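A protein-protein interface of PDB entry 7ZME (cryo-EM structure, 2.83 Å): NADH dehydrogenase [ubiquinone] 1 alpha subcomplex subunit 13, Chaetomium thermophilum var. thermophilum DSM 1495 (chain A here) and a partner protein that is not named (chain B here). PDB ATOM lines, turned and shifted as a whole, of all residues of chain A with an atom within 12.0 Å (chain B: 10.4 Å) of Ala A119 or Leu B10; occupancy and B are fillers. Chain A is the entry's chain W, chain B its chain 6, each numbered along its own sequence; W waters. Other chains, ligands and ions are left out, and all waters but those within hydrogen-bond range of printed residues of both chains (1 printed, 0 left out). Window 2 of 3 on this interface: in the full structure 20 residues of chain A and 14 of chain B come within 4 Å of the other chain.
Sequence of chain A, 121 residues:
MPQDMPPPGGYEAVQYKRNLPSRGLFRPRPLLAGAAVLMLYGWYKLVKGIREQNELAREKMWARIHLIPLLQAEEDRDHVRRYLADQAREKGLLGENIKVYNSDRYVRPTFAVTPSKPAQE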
ATOM      1  N   ARG A  82     -31.062 -39.541   5.587  1.00  0.00           N
ATOM      2  CA  ARG A  82     -29.628 -39.150   5.670  1.00  0.00           C
ATOM      3  C   ARG A  82     -28.718 -40.365   5.543  1.00  0.00           C
ATOM      4  O   ARG A  82     -27.629 -40.209   4.982  1.00  0.00           O
ATOM      5  CB  ARG A  82     -29.345 -38.231   6.862  1.00  0.00           C
ATOM      6  CG  ARG A  82     -30.116 -36.923   6.802  1.00  0.00           C
ATOM      7  CD  ARG A  82     -29.590 -35.861   7.740  1.00  0.00           C
ATOM      8  NE  ARG A  82     -28.251 -35.429   7.385  1.00  0.00           N
ATOM      9  CZ  ARG A  82     -27.672 -34.331   7.848  1.00  0.00           C
ATOM     10  NH1 ARG A  82     -26.447 -34.020   7.467  1.00  0.00           N
ATOM     11  NH2 ARG A  82     -28.322 -33.540   8.678  1.00  0.00           N
ATOM     12  N   ALA A 112     -19.616 -37.277  10.738  1.00  0.00           N
ATOM     13  CA  ALA A 112     -20.263 -37.022   9.435  1.00  0.00           C
ATOM     14  C   ALA A 112     -19.316 -36.280   8.504  1.00  0.00           C
ATOM     15  O   ALA A 112     -18.542 -35.460   9.005  1.00  0.00           O
ATOM     16  CB  ALA A 112     -21.534 -36.244   9.621  1.00  0.00           C
ATOM     17  N   VAL A 113     -19.359 -36.587   7.213  1.00  0.00           N
ATOM     18  CA  VAL A 113     -18.596 -35.845   6.220  1.00  0.00           C
ATOM     19  C   VAL A 113     -19.133 -34.422   6.153  1.00  0.00           C
ATOM     20  O   VAL A 113     -20.344 -34.205   6.030  1.00  0.00           O
ATOM     21  CB  VAL A 113     -18.679 -36.539   4.852  1.00  0.00           C
ATOM     22  CG1 VAL A 113     -18.362 -35.563   3.734  1.00  0.00           C
ATOM     23  CG2 VAL A 113     -17.756 -37.732   4.801  1.00  0.00           C
ATOM     24  N   THR A 114     -18.240 -33.445   6.243  1.00  0.00           N
ATOM     25  CA  THR A 114     -18.653 -32.056   6.145  1.00  0.00           C
ATOM     26  C   THR A 114     -17.867 -31.361   5.046  1.00  0.00           C
ATOM     27  O   THR A 114     -16.738 -31.756   4.736  1.00  0.00           O
ATOM     28  CB  THR A 114     -18.451 -31.302   7.472  1.00  0.00           C
ATOM     29  OG1 THR A 114     -17.073 -30.944   7.621  1.00  0.00           O
ATOM     30  CG2 THR A 114     -18.888 -32.149   8.655  1.00  0.00           C
ATOM     31  N   PRO A 115     -18.444 -30.333   4.430  1.00  0.00           N
ATOM     32  CA  PRO A 115     -17.703 -29.566   3.425  1.00  0.00           C
ATOM     33  C   PRO A 115     -16.589 -28.749   4.058  1.00  0.00           C
ATOM     34  O   PRO A 115     -16.570 -28.486   5.261  1.00  0.00           O
ATOM     35  CB  PRO A 115     -18.771 -28.662   2.804  1.00  0.00           C
ATOM     36  CG  PRO A 115     -19.877 -28.630   3.793  1.00  0.00           C
ATOM     37  CD  PRO A 115     -19.859 -29.939   4.495  1.00  0.00           C
ATOM     38  N   SER A 116     -15.645 -28.343   3.214  1.00  0.00           N
ATOM     39  CA  SER A 116     -14.462 -27.636   3.683  1.00  0.00           C
ATOM     40  C   SER A 116     -14.747 -26.202   4.099  1.00  0.00           C
ATOM     41  O   SER A 116     -13.868 -25.559   4.686  1.00  0.00           O
ATOM     42  CB  SER A 116     -13.382 -27.646   2.602  1.00  0.00           C
ATOM     43  OG  SER A 116     -12.359 -26.711   2.896  1.00  0.00           O
ATOM     44  N   LYS A 117     -15.939 -25.681   3.815  1.00  0.00           N
ATOM     45  CA  LYS A 117     -16.280 -24.315   4.161  1.00  0.00           C
ATOM     46  C   LYS A 117     -17.722 -24.245   4.639  1.00  0.00           C
ATOM     47  O   LYS A 117     -18.587 -24.951   4.102  1.00  0.00           O
ATOM     48  CB  LYS A 117     -16.087 -23.382   2.957  1.00  0.00           C
ATOM     49  CG  LYS A 117     -16.127 -21.902   3.291  1.00  0.00           C
ATOM     50  CD  LYS A 117     -15.870 -21.053   2.055  1.00  0.00           C
ATOM     51  CE  LYS A 117     -14.387 -20.982   1.732  1.00  0.00           C
ATOM     52  NZ  LYS A 117     -14.075 -19.860   0.806  1.00  0.00           N
ATOM     53  N   PRO A 118     -18.012 -23.414   5.640  1.00  0.00           N
ATOM     54  CA  PRO A 118     -19.413 -23.129   5.976  1.00  0.00           C
ATOM     55  C   PRO A 118     -20.048 -22.211   4.946  1.00  0.00           C
ATOM     56  O   PRO A 118     -19.404 -21.838   3.962  1.00  0.00           O
ATOM     57  CB  PRO A 118     -19.323 -22.456   7.351  1.00  0.00           C
ATOM     58  CG  PRO A 118     -17.945 -22.754   7.851  1.00  0.00           C
ATOM     59  CD  PRO A 118     -17.086 -22.862   6.638  1.00  0.00           C
ATOM     60  N   ALA A 119     -21.307 -21.842   5.157  1.00  0.00           N
ATOM     61  CA  ALA A 119     -21.962 -20.920   4.240  1.00  0.00           C
ATOM     62  C   ALA A 119     -21.288 -19.554   4.293  1.00  0.00           C
ATOM     63  O   ALA A 119     -20.841 -19.103   5.350  1.00  0.00           O
ATOM     64  CB  ALA A 119     -23.445 -20.802   4.579  1.00  0.00           C
ATOM     65  N   GLN A 120     -21.215 -18.893   3.135  1.00  0.00           N
ATOM     66  CA  GLN A 120     -20.442 -17.661   3.021  1.00  0.00           C
ATOM     67  C   GLN A 120     -21.031 -16.512   3.830  1.00  0.00           C
ATOM     68  O   GLN A 120     -20.278 -15.629   4.255  1.00  0.00           O
ATOM     69  CB  GLN A 120     -20.323 -17.251   1.553  1.00  0.00           C
ATOM     70  CG  GLN A 120     -19.196 -16.267   1.273  1.00  0.00           C
ATOM     71  CD  GLN A 120     -17.917 -16.614   2.012  1.00  0.00           C
ATOM     72  OE1 GLN A 120     -17.429 -17.742   1.941  1.00  0.00           O
ATOM     73  NE2 GLN A 120     -17.368 -15.640   2.730  1.00  0.00           N
ATOM     74  N   GLU A 121     -22.343 -16.504   4.048  1.00  0.00           N
ATOM     75  CA  GLU A 121     -23.015 -15.435   4.789  1.00  0.00           C
ATOM     76  C   GLU A 121     -22.755 -14.065   4.171  1.00  0.00           C
ATOM     77  O   GLU A 121     -23.587 -13.162   4.268  1.00  0.00           O
ATOM     78  CB  GLU A 121     -22.579 -15.438   6.258  1.00  0.00           C
ATOM     79  N   ILE B   5     -24.802 -29.313  -4.451  1.00  0.00           N
ATOM     80  CA  ILE B   5     -23.945 -29.626  -3.267  1.00  0.00           C
ATOM     81  C   ILE B   5     -24.663 -30.702  -2.456  1.00  0.00           C
ATOM     82  O   ILE B   5     -24.136 -31.834  -2.419  1.00  0.00           O
ATOM     83  CB  ILE B   5     -23.700 -28.362  -2.422  1.00  0.00           C
ATOM     84  N   LEU B   7     -24.819 -31.040   0.718  1.00  0.00           N
ATOM     85  CA  LEU B   7     -24.301 -31.078   2.110  1.00  0.00           C
ATOM     86  C   LEU B   7     -23.996 -29.637   2.495  1.00  0.00           C
ATOM     87  O   LEU B   7     -23.039 -29.078   1.941  1.00  0.00           O
ATOM     88  CB  LEU B   7     -23.075 -31.990   2.222  1.00  0.00           C
ATOM     89  CG  LEU B   7     -23.364 -33.423   2.658  1.00  0.00           C
ATOM     90  CD1 LEU B   7     -22.070 -34.160   2.951  1.00  0.00           C
ATOM     91  CD2 LEU B   7     -24.271 -33.443   3.877  1.00  0.00           C
ATOM     92  N   LEU B   8     -24.786 -29.062   3.400  1.00  0.00           N
ATOM     93  CA  LEU B   8     -24.622 -27.615   3.666  1.00  0.00           C
ATOM     94  C   LEU B   8     -24.085 -27.366   5.073  1.00  0.00           C
ATOM     95  O   LEU B   8     -24.731 -27.803   6.037  1.00  0.00           O
ATOM     96  CB  LEU B   8     -25.974 -26.936   3.448  1.00  0.00           C
ATOM     97  CG  LEU B   8     -26.738 -27.385   2.204  1.00  0.00           C
ATOM     98  CD1 LEU B   8     -28.207 -27.009   2.298  1.00  0.00           C
ATOM     99  CD2 LEU B   8     -26.114 -26.811   0.944  1.00  0.00           C
ATOM    100  N   LEU B   9     -22.905 -26.656   5.147  1.00  0.00           N
ATOM    101  CA  LEU B   9     -22.393 -26.321   6.493  1.00  0.00           C
ATOM    102  C   LEU B   9     -22.956 -24.950   6.841  1.00  0.00           C
ATOM    103  O   LEU B   9     -23.114 -24.129   5.934  1.00  0.00           O
ATOM    104  CB  LEU B   9     -20.865 -26.376   6.549  1.00  0.00           C
ATOM    105  CG  LEU B   9     -20.267 -26.503   7.949  1.00  0.00           C
ATOM    106  CD1 LEU B   9     -20.903 -27.654   8.711  1.00  0.00           C
ATOM    107  CD2 LEU B   9     -18.760 -26.688   7.871  1.00  0.00           C
ATOM    108  N   LEU B  10     -23.284 -24.741   8.100  1.00  0.00           N
ATOM    109  CA  LEU B  10     -23.869 -23.490   8.542  1.00  0.00           C
ATOM    110  C   LEU B  10     -23.394 -23.192   9.952  1.00  0.00           C
ATOM    111  O   LEU B  10     -22.976 -24.087  10.685  1.00  0.00           O
ATOM    112  CB  LEU B  10     -25.397 -23.564   8.481  1.00  0.00           C
ATOM    113  CG  LEU B  10     -26.188 -22.265   8.538  1.00  0.00           C
ATOM    114  CD1 LEU B  10     -26.258 -21.635   7.175  1.00  0.00           C
ATOM    115  CD2 LEU B  10     -27.575 -22.564   9.059  1.00  0.00           C
ATOM    116  N   LYS B  11     -23.459 -21.919  10.325  1.00  0.00           N
ATOM    117  CA  LYS B  11     -23.144 -21.498  11.681  1.00  0.00           C
ATOM    118  C   LYS B  11     -24.416 -21.486  12.514  1.00  0.00           C
ATOM    119  O   LYS B  11     -25.452 -20.986  12.068  1.00  0.00           O
ATOM    120  CB  LYS B  11     -22.490 -20.117  11.683  1.00  0.00           C
ATOM    121  CG  LYS B  11     -21.088 -20.096  11.097  1.00  0.00           C
ATOM    122  CD  LYS B  11     -20.151 -19.239  11.931  1.00  0.00           C
ATOM    123  CE  LYS B  11     -18.720 -19.332  11.423  1.00  0.00           C
ATOM    124  NZ  LYS B  11     -17.847 -18.295  12.035  1.00  0.00           N
ATOM    125  N   GLU B  12     -24.335 -22.041  13.717  1.00  0.00           N
ATOM    126  CA  GLU B  12     -25.462 -22.047  14.639  1.00  0.00           C
ATOM    127  C   GLU B  12     -25.591 -20.672  15.287  1.00  0.00           C
ATOM    128  O   GLU B  12     -24.670 -20.214  15.967  1.00  0.00           O
ATOM    129  CB  GLU B  12     -25.263 -23.134  15.692  1.00  0.00           C
ATOM    130  CG  GLU B  12     -26.545 -23.658  16.295  1.00  0.00           C
ATOM    131  CD  GLU B  12     -26.331 -24.933  17.078  1.00  0.00           C
ATOM    132  OE1 GLU B  12     -27.273 -25.377  17.764  1.00  0.00           O
ATOM    133  OE2 GLU B  12     -25.217 -25.493  17.004  1.00  0.00           O
ATOM    134  N   ILE B  13     -26.736 -20.018  15.084  1.00  0.00           N
ATOM    135  CA  ILE B  13     -26.886 -18.629  15.506  1.00  0.00           C
ATOM    136  C   ILE B  13     -27.112 -18.533  17.010  1.00  0.00           C
ATOM    137  O   ILE B  13     -26.388 -17.821  17.714  1.00  0.00           O
ATOM    138  CB  ILE B  13     -28.008 -17.940  14.702  1.00  0.00           C
ATOM    139  CG1 ILE B  13     -28.190 -16.491  15.164  1.00  0.00           C
ATOM    140  CG2 ILE B  13     -29.315 -18.738  14.744  1.00  0.00           C
ATOM    141  CD1 ILE B  13     -29.053 -15.660  14.242  1.00  0.00           C
ATOM    142  N   TYR B  14     -28.114 -19.230  17.525  1.00  0.00           N
ATOM    143  CA  TYR B  14     -28.299 -19.419  18.955  1.00  0.00           C
ATOM    144  C   TYR B  14     -28.136 -20.900  19.261  1.00  0.00           C
ATOM    145  O   TYR B  14     -27.874 -21.711  18.372  1.00  0.00           O
ATOM    146  CB  TYR B  14     -29.667 -18.910  19.419  1.00  0.00           C
ATOM    147  CG  TYR B  14     -29.946 -17.457  19.104  1.00  0.00           C
ATOM    148  CD1 TYR B  14     -30.450 -17.076  17.870  1.00  0.00           C
ATOM    149  CD2 TYR B  14     -29.715 -16.468  20.047  1.00  0.00           C
ATOM    150  CE1 TYR B  14     -30.705 -15.753  17.584  1.00  0.00           C
ATOM    151  CE2 TYR B  14     -29.969 -15.142  19.768  1.00  0.00           C
ATOM    152  CZ  TYR B  14     -30.464 -14.790  18.536  1.00  0.00           C
ATOM    153  OH  TYR B  14     -30.719 -13.467  18.260  1.00  0.00           O
ATOM    154  N   THR B  15     -28.285 -21.253  20.532  1.00  0.00           N
ATOM    155  CA  THR B  15     -28.262 -22.635  20.999  1.00  0.00           C
ATOM    156  C   THR B  15     -26.933 -23.333  20.717  1.00  0.00           C
ATOM    157  O   THR B  15     -26.802 -24.534  20.982  1.00  0.00           O
ATOM    158  CB  THR B  15     -29.419 -23.457  20.408  1.00  0.00           C
ATOM    159  OG1 THR B  15     -29.309 -23.502  18.981  1.00  0.00           O
ATOM    160  CG2 THR B  15     -30.753 -22.832  20.776  1.00  0.00           C
ATOM    161  N   ASN B  16     -25.948 -22.615  20.188  1.00  0.00           N
ATOM    162  CA  ASN B  16     -24.621 -23.175  20.013  1.00  0.00           C
ATOM    163  C   ASN B  16     -23.930 -23.346  21.363  1.00  0.00           C
ATOM    164  O   ASN B  16     -24.281 -22.711  22.361  1.00  0.00           O
ATOM    165  CB  ASN B  16     -23.786 -22.292  19.087  1.00  0.00           C
ATOM    166  CG  ASN B  16     -23.699 -20.859  19.561  1.00  0.00           C
ATOM    167  OD1 ASN B  16     -24.217 -20.504  20.617  1.00  0.00           O
ATOM    168  ND2 ASN B  16     -23.033 -20.024  18.779  1.00  0.00           N
ATOM    169  N   PHE B 168     -15.436 -34.380  12.239  1.00  0.00           N
ATOM    170  CA  PHE B 168     -16.404 -33.567  13.012  1.00  0.00           C
ATOM    171  C   PHE B 168     -17.441 -34.498  13.629  1.00  0.00           C
ATOM    172  O   PHE B 168     -17.981 -35.365  12.924  1.00  0.00           O
ATOM    173  CB  PHE B 168     -17.061 -32.506  12.131  1.00  0.00           C
ATOM    174  CG  PHE B 168     -16.132 -31.383  11.747  1.00  0.00           C
ATOM    175  CD1 PHE B 168     -15.944 -30.302  12.592  1.00  0.00           C
ATOM    176  CD2 PHE B 168     -15.428 -31.419  10.556  1.00  0.00           C
ATOM    177  CE1 PHE B 168     -15.079 -29.277  12.248  1.00  0.00           C
ATOM    178  CE2 PHE B 168     -14.565 -30.392  10.212  1.00  0.00           C
ATOM    179  CZ  PHE B 168     -14.393 -29.322  11.059  1.00  0.00           C
ATOM    180  N   ILE B 170     -20.982 -35.582  15.007  1.00  0.00           N
ATOM    181  CA  ILE B 170     -22.363 -35.224  14.572  1.00  0.00           C
ATOM    182  C   ILE B 170     -23.360 -35.739  15.615  1.00  0.00           C
ATOM    183  O   ILE B 170     -23.224 -36.893  16.039  1.00  0.00           O
ATOM    184  CB  ILE B 170     -22.635 -35.719  13.136  1.00  0.00           C
ATOM    185  CG1 ILE B 170     -23.861 -35.045  12.519  1.00  0.00           C
ATOM    186  CG2 ILE B 170     -22.707 -37.232  13.046  1.00  0.00           C
ATOM    187  CD1 ILE B 170     -23.598 -33.654  12.011  1.00  0.00           C
HETATM  188  O   HOH W   1     -16.045 -34.507   9.390  1.00  0.00           O
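Of the 13 printed residues of chain B, 5 touch a printed residue of chain A. Hydrophobic or aromatic side chains of chain A within 4 Å of the printed part of chain B: Ala A112, Pro A115 and Ala A119. Among the printed residues, 10 pairs touch across the chains. Among the printed residues, no Asp or Glu carboxylate lies within 4 Å of a Lys or Arg side-chain nitrogen of the other chain.
Water W1 bridges O of Ala A112 (2.7 Å) and N of Phe B168 (2.9 Å).
Ala A112 touches Ile B170 (CB to CB, 3.7 Å). O of Val A113 touches CD1 of Leu B7, 3.5 Å away. OG1 of Thr A114 touches CD2 of Phe B168 (3.4 Å). Pro A115 touches Leu B7. CB of Leu B9 touches CG of Pro A115 (3.7 Å). CB of Leu B9 touches O of Lys A117, at 3.6 Å. Pro A118 touches Leu B9. CB of Ala A119 touches CD1 of Leu B10 (3.9 Å).
Of the printed residues of chain B, Ala A112 touches Phe B168 (3.3 Å) and Ile B170 (3.7 Å). Of the printed residues of chain B, Lys A117 touches Leu B9. Printed residues of chain B within 4 Å of Pro A118: Leu B9 (3.6 Å). No residue of chain B comes within 4 Å of Gln A120. No residue of chain A comes within 4 Å of Leu B8. Of chain A, only Ala A119 comes within 4 Å of Leu B10. No residue of chain A comes within 4 Å of Lys B11. Thr B15 touches none of the printed residues of chain A. The nearest residue of chain B that does not touch Ala A119 is Lys B11 (5.6 Å). The nearest printed residue of chain A that does not touch Leu B7 is Arg A82 (4.2 Å).
The backbone carbonyl oxygen of Phe B168 is in hydrogen-bond range of the backbone NH of Ala A112, at 3.3 Å. N of Ala A119 sits at hydrogen-bond distance from O of Leu B9 (3.0 Å).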
